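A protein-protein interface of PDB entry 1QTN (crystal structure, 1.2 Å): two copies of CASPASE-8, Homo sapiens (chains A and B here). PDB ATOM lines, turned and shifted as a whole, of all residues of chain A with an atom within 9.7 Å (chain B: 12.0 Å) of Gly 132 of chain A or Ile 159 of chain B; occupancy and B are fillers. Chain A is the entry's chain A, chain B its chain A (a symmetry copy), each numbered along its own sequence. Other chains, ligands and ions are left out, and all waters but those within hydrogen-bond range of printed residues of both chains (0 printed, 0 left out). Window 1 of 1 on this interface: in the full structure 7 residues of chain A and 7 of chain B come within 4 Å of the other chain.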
ATOM      1  N   GLN A  90      32.731   0.225 -17.345  1.00  0.00           N
ATOM      2  CA  GLN A  90      31.329   0.635 -17.458  1.00  0.00           C
ATOM      3  C   GLN A  90      31.206   2.158 -17.524  1.00  0.00           C
ATOM      4  O   GLN A  90      30.316   2.671 -18.184  1.00  0.00           O
ATOM      5  CB  GLN A  90      30.592   0.103 -16.223  1.00  0.00           C
ATOM      6  CG  GLN A  90      29.219   0.673 -15.972  1.00  0.00           C
ATOM      7  CD  GLN A  90      28.721   0.225 -14.600  1.00  0.00           C
ATOM      8  OE1 GLN A  90      28.058  -0.791 -14.513  1.00  0.00           O
ATOM      9  NE2 GLN A  90      29.163   0.931 -13.576  1.00  0.00           N
ATOM     10  N   THR A 127      28.125  -9.561 -16.570  1.00  0.00           N
ATOM     11  CA  THR A 127      27.620  -9.063 -17.841  1.00  0.00           C
ATOM     12  C   THR A 127      26.685  -7.873 -17.651  1.00  0.00           C
ATOM     13  O   THR A 127      26.661  -6.980 -18.489  1.00  0.00           O
ATOM     14  CB  THR A 127      26.898 -10.166 -18.632  1.00  0.00           C
ATOM     15  OG1 THR A 127      25.830 -10.675 -17.833  1.00  0.00           O
ATOM     16  CG2 THR A 127      27.845 -11.337 -18.912  1.00  0.00           C
ATOM     17  N   SER A 128      25.917  -7.865 -16.575  1.00  0.00           N
ATOM     18  CA  SER A 128      24.923  -6.847 -16.327  1.00  0.00           C
ATOM     19  C   SER A 128      25.519  -5.482 -16.119  1.00  0.00           C
ATOM     20  O   SER A 128      24.791  -4.467 -16.179  1.00  0.00           O
ATOM     21  CB  SER A 128      23.957  -7.249 -15.234  1.00  0.00           C
ATOM     22  OG  SER A 128      24.580  -7.194 -13.954  1.00  0.00           O
ATOM     23  N   GLN A 129      26.832  -5.369 -15.902  1.00  0.00           N
ATOM     24  CA  GLN A 129      27.464  -4.069 -15.778  1.00  0.00           C
ATOM     25  C   GLN A 129      27.546  -3.339 -17.097  1.00  0.00           C
ATOM     26  O   GLN A 129      27.818  -2.121 -17.120  1.00  0.00           O
ATOM     27  CB  GLN A 129      28.850  -4.167 -15.147  1.00  0.00           C
ATOM     28  CG  GLN A 129      28.943  -4.878 -13.836  1.00  0.00           C
ATOM     29  CD  GLN A 129      27.858  -4.491 -12.857  1.00  0.00           C
ATOM     30  OE1 GLN A 129      27.204  -5.331 -12.249  1.00  0.00           O
ATOM     31  NE2 GLN A 129      27.684  -3.187 -12.696  1.00  0.00           N
ATOM     32  N   PHE A 130      27.196  -3.996 -18.214  1.00  0.00           N
ATOM     33  CA  PHE A 130      27.321  -3.436 -19.519  1.00  0.00           C
ATOM     34  C   PHE A 130      26.040  -3.331 -20.322  1.00  0.00           C
ATOM     35  O   PHE A 130      26.043  -3.147 -21.530  1.00  0.00           O
ATOM     36  CB  PHE A 130      28.425  -4.116 -20.359  1.00  0.00           C
ATOM     37  CG  PHE A 130      29.785  -3.980 -19.658  1.00  0.00           C
ATOM     38  CD1 PHE A 130      30.567  -2.857 -19.939  1.00  0.00           C
ATOM     39  CD2 PHE A 130      30.194  -4.892 -18.733  1.00  0.00           C
ATOM     40  CE1 PHE A 130      31.772  -2.687 -19.237  1.00  0.00           C
ATOM     41  CE2 PHE A 130      31.386  -4.720 -18.035  1.00  0.00           C
ATOM     42  CZ  PHE A 130      32.141  -3.596 -18.276  1.00  0.00           C
ATOM     43  N   THR A 131      24.923  -3.408 -19.601  1.00  0.00           N
ATOM     44  CA  THR A 131      23.622  -3.195 -20.251  1.00  0.00           C
ATOM     45  C   THR A 131      23.588  -1.772 -20.812  1.00  0.00           C
ATOM     46  O   THR A 131      24.393  -0.909 -20.485  1.00  0.00           O
ATOM     47  CB  THR A 131      22.471  -3.359 -19.248  1.00  0.00           C
ATOM     48  OG1 THR A 131      22.572  -2.376 -18.251  1.00  0.00           O
ATOM     49  CG2 THR A 131      22.373  -4.727 -18.652  1.00  0.00           C
ATOM     50  N   GLY A 132      22.598  -1.543 -21.664  1.00  0.00           N
ATOM     51  CA  GLY A 132      22.516  -0.222 -22.291  1.00  0.00           C
ATOM     52  C   GLY A 132      22.281   0.882 -21.280  1.00  0.00           C
ATOM     53  O   GLY A 132      22.750   2.021 -21.526  1.00  0.00           O
ATOM     54  N   LEU A 133      21.578   0.629 -20.207  1.00  0.00           N
ATOM     55  CA  LEU A 133      21.365   1.664 -19.185  1.00  0.00           C
ATOM     56  C   LEU A 133      22.642   1.950 -18.427  1.00  0.00           C
ATOM     57  O   LEU A 133      22.900   3.096 -18.009  1.00  0.00           O
ATOM     58  CB  LEU A 133      20.243   1.312 -18.257  1.00  0.00           C
ATOM     59  CG  LEU A 133      18.835   1.235 -18.898  1.00  0.00           C
ATOM     60  CD1 LEU A 133      17.853   0.589 -17.942  1.00  0.00           C
ATOM     61  CD2 LEU A 133      18.340   2.620 -19.308  1.00  0.00           C
ATOM     62  N   LYS A 134      23.394   0.905 -18.118  1.00  0.00           N
ATOM     63  CA  LYS A 134      24.590   1.075 -17.252  1.00  0.00           C
ATOM     64  C   LYS A 134      25.755   1.579 -18.043  1.00  0.00           C
ATOM     65  O   LYS A 134      26.657   2.225 -17.447  1.00  0.00           O
ATOM     66  CB  LYS A 134      24.866  -0.240 -16.518  1.00  0.00           C
ATOM     67  CG  LYS A 134      23.737  -0.583 -15.550  1.00  0.00           C
ATOM     68  CD  LYS A 134      24.221  -1.280 -14.305  1.00  0.00           C
ATOM     69  CE  LYS A 134      23.141  -1.331 -13.230  1.00  0.00           C
ATOM     70  NZ  LYS A 134      23.219  -0.168 -12.297  1.00  0.00           N
ATOM     71  N   CYS A 135      25.804   1.307 -19.334  1.00  0.00           N
ATOM     72  CA  CYS A 135      26.850   1.771 -20.219  1.00  0.00           C
ATOM     73  C   CYS A 135      26.274   2.236 -21.540  1.00  0.00           C
ATOM     74  O   CYS A 135      26.301   1.590 -22.582  1.00  0.00           O
ATOM     75  CB  CYS A 135      27.910   0.700 -20.440  1.00  0.00           C
ATOM     76  SG  CYS A 135      29.375   1.281 -21.294  1.00  0.00           S
ATOM     77  N   PRO A 136      25.712   3.480 -21.506  1.00  0.00           N
ATOM     78  CA  PRO A 136      25.023   3.999 -22.661  1.00  0.00           C
ATOM     79  C   PRO A 136      25.838   4.169 -23.905  1.00  0.00           C
ATOM     80  O   PRO A 136      25.329   4.062 -25.027  1.00  0.00           O
ATOM     81  CB  PRO A 136      24.425   5.351 -22.204  1.00  0.00           C
ATOM     82  CG  PRO A 136      24.326   5.177 -20.707  1.00  0.00           C
ATOM     83  CD  PRO A 136      25.532   4.353 -20.321  1.00  0.00           C
ATOM     84  N   SER A 137      27.150   4.411 -23.768  1.00  0.00           N
ATOM     85  CA  SER A 137      27.998   4.536 -24.922  1.00  0.00           C
ATOM     86  C   SER A 137      28.263   3.220 -25.640  1.00  0.00           C
ATOM     87  O   SER A 137      28.879   3.270 -26.732  1.00  0.00           O
ATOM     88  CB  SER A 137      29.308   5.262 -24.609  1.00  0.00           C
ATOM     89  OG  SER A 137      30.101   4.594 -23.714  1.00  0.00           O
ATOM     90  N   LEU A 138      27.827   2.092 -25.119  1.00  0.00           N
ATOM     91  CA  LEU A 138      27.813   0.824 -25.838  1.00  0.00           C
ATOM     92  C   LEU A 138      26.408   0.443 -26.258  1.00  0.00           C
ATOM     93  O   LEU A 138      26.200  -0.650 -26.803  1.00  0.00           O
ATOM     94  CB  LEU A 138      28.459  -0.296 -25.032  1.00  0.00           C
ATOM     95  CG  LEU A 138      29.973  -0.217 -24.838  1.00  0.00           C
ATOM     96  CD1 LEU A 138      30.412  -1.247 -23.792  1.00  0.00           C
ATOM     97  CD2 LEU A 138      30.683  -0.430 -26.179  1.00  0.00           C
ATOM     98  N   ALA A 139      25.401   1.303 -26.079  1.00  0.00           N
ATOM     99  CA  ALA A 139      24.045   0.942 -26.488  1.00  0.00           C
ATOM    100  C   ALA A 139      23.965   0.681 -27.953  1.00  0.00           C
ATOM    101  O   ALA A 139      24.482   1.469 -28.788  1.00  0.00           O
ATOM    102  CB  ALA A 139      23.056   2.021 -26.061  1.00  0.00           C
ATOM    103  N   GLY A 140      23.340  -0.437 -28.362  1.00  0.00           N
ATOM    104  CA  GLY A 140      23.241  -0.832 -29.740  1.00  0.00           C
ATOM    105  C   GLY A 140      24.487  -1.508 -30.301  1.00  0.00           C
ATOM    106  O   GLY A 140      24.486  -1.862 -31.482  1.00  0.00           O
ATOM    107  N   LYS A 141      25.530  -1.623 -29.492  1.00  0.00           N
ATOM    108  CA  LYS A 141      26.793  -2.213 -29.906  1.00  0.00           C
ATOM    109  C   LYS A 141      26.978  -3.583 -29.234  1.00  0.00           C
ATOM    110  O   LYS A 141      26.604  -3.773 -28.082  1.00  0.00           O
ATOM    111  CB  LYS A 141      27.959  -1.307 -29.556  1.00  0.00           C
ATOM    112  CG  LYS A 141      27.812   0.114 -30.110  1.00  0.00           C
ATOM    113  CD  LYS A 141      28.947   1.003 -29.627  1.00  0.00           C
ATOM    114  CE  LYS A 141      28.748   2.428 -30.099  1.00  0.00           C
ATOM    115  NZ  LYS A 141      29.750   3.337 -29.465  1.00  0.00           N
ATOM    116  N   LYS A 143      28.425  -6.586 -27.232  1.00  0.00           N
ATOM    117  CA  LYS A 143      29.177  -6.822 -26.020  1.00  0.00           C
ATOM    118  C   LYS A 143      29.369  -8.341 -25.894  1.00  0.00           C
ATOM    119  O   LYS A 143      28.400  -9.095 -25.829  1.00  0.00           O
ATOM    120  CB  LYS A 143      28.443  -6.277 -24.803  1.00  0.00           C
ATOM    121  CG  LYS A 143      28.272  -4.744 -25.010  1.00  0.00           C
ATOM    122  CD  LYS A 143      27.232  -4.141 -24.199  1.00  0.00           C
ATOM    123  CE  LYS A 143      25.822  -4.265 -24.737  1.00  0.00           C
ATOM    124  NZ  LYS A 143      25.496  -3.138 -25.657  1.00  0.00           N
ATOM    125  N   TYR B 155       9.532  -6.141 -15.867  1.00  0.00           N
ATOM    126  CA  TYR B 155       9.444  -5.635 -17.231  1.00  0.00           C
ATOM    127  C   TYR B 155      10.872  -5.255 -17.666  1.00  0.00           C
ATOM    128  O   TYR B 155      11.517  -4.441 -17.021  1.00  0.00           O
ATOM    129  CB  TYR B 155       8.580  -4.347 -17.249  1.00  0.00           C
ATOM    130  CG  TYR B 155       7.128  -4.627 -16.933  1.00  0.00           C
ATOM    131  CD1 TYR B 155       6.311  -5.294 -17.811  1.00  0.00           C
ATOM    132  CD2 TYR B 155       6.574  -4.202 -15.712  1.00  0.00           C
ATOM    133  CE1 TYR B 155       4.972  -5.570 -17.523  1.00  0.00           C
ATOM    134  CE2 TYR B 155       5.248  -4.493 -15.412  1.00  0.00           C
ATOM    135  CZ  TYR B 155       4.464  -5.164 -16.315  1.00  0.00           C
ATOM    136  OH  TYR B 155       3.130  -5.434 -16.019  1.00  0.00           O
ATOM    137  N   GLN B 156      11.311  -5.791 -18.781  1.00  0.00           N
ATOM    138  CA  GLN B 156      12.586  -5.395 -19.385  1.00  0.00           C
ATOM    139  C   GLN B 156      12.476  -3.942 -19.829  1.00  0.00           C
ATOM    140  O   GLN B 156      11.569  -3.559 -20.563  1.00  0.00           O
ATOM    141  CB  GLN B 156      12.833  -6.343 -20.558  1.00  0.00           C
ATOM    142  CG  GLN B 156      14.024  -6.094 -21.393  1.00  0.00           C
ATOM    143  CD  GLN B 156      15.341  -6.505 -20.761  1.00  0.00           C
ATOM    144  OE1 GLN B 156      15.445  -7.148 -19.717  1.00  0.00           O
ATOM    145  NE2 GLN B 156      16.358  -6.051 -21.381  1.00  0.00           N
ATOM    146  N   LYS B 157      13.453  -3.135 -19.427  1.00  0.00           N
ATOM    147  CA  LYS B 157      13.450  -1.723 -19.786  1.00  0.00           C
ATOM    148  C   LYS B 157      13.995  -1.499 -21.174  1.00  0.00           C
ATOM    149  O   LYS B 157      14.704  -2.367 -21.718  1.00  0.00           O
ATOM    150  CB  LYS B 157      14.289  -0.932 -18.774  1.00  0.00           C
ATOM    151  CG  LYS B 157      13.705  -0.905 -17.372  1.00  0.00           C
ATOM    152  CD  LYS B 157      14.712  -0.335 -16.388  1.00  0.00           C
ATOM    153  CE  LYS B 157      14.181  -0.257 -14.969  1.00  0.00           C
ATOM    154  NZ  LYS B 157      14.134  -1.586 -14.305  1.00  0.00           N
ATOM    155  N   GLY B 158      13.696  -0.337 -21.729  1.00  0.00           N
ATOM    156  CA  GLY B 158      14.198   0.043 -23.032  1.00  0.00           C
ATOM    157  C   GLY B 158      15.337   1.056 -22.947  1.00  0.00           C
ATOM    158  O   GLY B 158      15.482   1.713 -21.913  1.00  0.00           O
ATOM    159  N   ILE B 159      16.126   1.110 -23.992  1.00  0.00           N
ATOM    160  CA  ILE B 159      17.243   2.018 -24.166  1.00  0.00           C
ATOM    161  C   ILE B 159      17.161   2.669 -25.536  1.00  0.00           C
ATOM    162  O   ILE B 159      16.781   2.040 -26.516  1.00  0.00           O
ATOM    163  CB  ILE B 159      18.620   1.275 -24.057  1.00  0.00           C
ATOM    164  CG1 ILE B 159      18.752   0.109 -25.042  1.00  0.00           C
ATOM    165  CG2 ILE B 159      18.791   0.781 -22.631  1.00  0.00           C
ATOM    166  CD1 ILE B 159      20.091  -0.598 -25.041  1.00  0.00           C
ATOM    167  N   PRO B 160      17.488   3.979 -25.594  1.00  0.00           N
ATOM    168  CA  PRO B 160      17.388   4.688 -26.871  1.00  0.00           C
ATOM    169  C   PRO B 160      18.580   4.448 -27.768  1.00  0.00           C
ATOM    170  O   PRO B 160      19.739   4.442 -27.316  1.00  0.00           O
ATOM    171  CB  PRO B 160      17.338   6.166 -26.432  1.00  0.00           C
ATOM    172  CG  PRO B 160      18.115   6.192 -25.168  1.00  0.00           C
ATOM    173  CD  PRO B 160      17.838   4.876 -24.463  1.00  0.00           C
ATOM    174  N   VAL B 161      18.313   4.203 -29.040  1.00  0.00           N
ATOM    175  CA  VAL B 161      19.381   4.024 -30.025  1.00  0.00           C
ATOM    176  C   VAL B 161      18.989   4.690 -31.340  1.00  0.00           C
ATOM    177  O   VAL B 161      17.824   5.037 -31.516  1.00  0.00           O
ATOM    178  CB  VAL B 161      19.645   2.535 -30.297  1.00  0.00           C
ATOM    179  CG1 VAL B 161      20.273   1.864 -29.115  1.00  0.00           C
ATOM    180  CG2 VAL B 161      18.404   1.819 -30.785  1.00  0.00           C
ATOM    181  N   GLU B 162      19.998   4.918 -32.176  1.00  0.00           N
ATOM    182  CA  GLU B 162      19.725   5.550 -33.481  1.00  0.00           C
ATOM    183  C   GLU B 162      19.041   4.553 -34.405  1.00  0.00           C
ATOM    184  O   GLU B 162      19.202   3.341 -34.247  1.00  0.00           O
ATOM    185  CB  GLU B 162      21.005   6.084 -34.095  1.00  0.00           C
ATOM    186  CG  GLU B 162      21.190   7.594 -33.906  1.00  0.00           C
ATOM    187  CD  GLU B 162      22.616   8.010 -34.238  1.00  0.00           C
ATOM    188  OE1 GLU B 162      23.506   7.130 -34.206  1.00  0.00           O
ATOM    189  OE2 GLU B 162      22.826   9.196 -34.557  1.00  0.00           O
ATOM    190  N   THR B 163      18.187   5.061 -35.286  1.00  0.00           N
ATOM    191  CA  THR B 163      17.416   4.211 -36.189  1.00  0.00           C
ATOM    192  C   THR B 163      18.300   3.673 -37.317  1.00  0.00           C
ATOM    193  O   THR B 163      19.047   4.434 -37.924  1.00  0.00           O
ATOM    194  CB  THR B 163      16.279   5.042 -36.864  1.00  0.00           C
ATOM    195  OG1 THR B 163      15.624   5.799 -35.823  1.00  0.00           O
ATOM    196  CG2 THR B 163      15.227   4.084 -37.414  1.00  0.00           C
ATOM    197  N   ASP B 164      18.164   2.378 -37.601  1.00  0.00           N
ATOM    198  CA  ASP B 164      18.940   1.780 -38.689  1.00  0.00           C
ATOM    199  C   ASP B 164      18.502   2.360 -40.051  1.00  0.00           C
ATOM    200  O   ASP B 164      17.325   2.752 -40.163  1.00  0.00           O
ATOM    201  CB  ASP B 164      18.745   0.277 -38.732  1.00  0.00           C
ATOM    202  CG  ASP B 164      19.500  -0.477 -37.655  1.00  0.00           C
ATOM    203  OD1 ASP B 164      18.954  -1.509 -37.217  1.00  0.00           O
ATOM    204  OD2 ASP B 164      20.600  -0.037 -37.249  1.00  0.00           O
ATOM    205  OXT ASP B 164      19.272   2.198 -41.021  1.00  0.00           O
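No position is printed for both chains.
Among the printed residues, pairs that only touch across the chains: Leu 133 of chain A with Lys 157 of chain B (3.6 Å), Gly 132 of chain A with Ile 159 of chain B (3.7 Å), Leu 133 of chain A with Ile 159 of chain B (3.7 Å), Gly 140 of chain A with Val 161 of chain B (3.9 Å) and Leu 133 of chain A with Gly 158 of chain B (3.97 Å).
No residue of chain B comes within 4 Å of Thr 131 of chain A.
Gly 132 of chain A touches just one residue of chain B: Ile 159.
Of chain B, only Lys 157 (3.6 Å), Gly 158 (3.97 Å) and Ile 159 (3.7 Å) come within 4 Å of Leu 133 of chain A.
No residue of chain B comes within 4 Å of Cys 135 of chain A.
No residue of chain B comes within 4 Å of Ala 139 of chain A.
Gln 156 of chain B touches none of the printed residues of chain A.
Of the printed residues of chain A, Lys 157 of chain B touches Leu 133 (3.6 Å).
Of chain A, only Leu 133 (3.97 Å) comes within 4 Å of Gly 158 of chain B.
Ile 159 of chain B touches two residues of chain A.
Printed residues of chain A within 4 Å of Val 161 of chain B: Gly 140 (3.9 Å).
The nearest residue of chain B that does not touch Gly 132 of chain A is Pro 160 of chain B (6.4 Å).
The nearest printed residue of chain A that does not touch Val 161 of chain B is Ala 139 of chain A (4.05 Å).
Printed residues of chain A that touch a printed residue of chain B: Gly 132, Leu 133 and Gly 140.
Hydrophobic or aromatic side chains of chain A within 4 Å of the printed part of chain B: Leu 133.
Printed residues of chain B that touch a printed residue of chain A: Lys 157, Gly 158, Ile 159 and Val 161.
Among the printed residues, 5 pairs touch across the chains.
Among the printed residues, no Asp or Glu carboxylate lies within 4 Å of a Lys or Arg side-chain nitrogen of the other chain.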
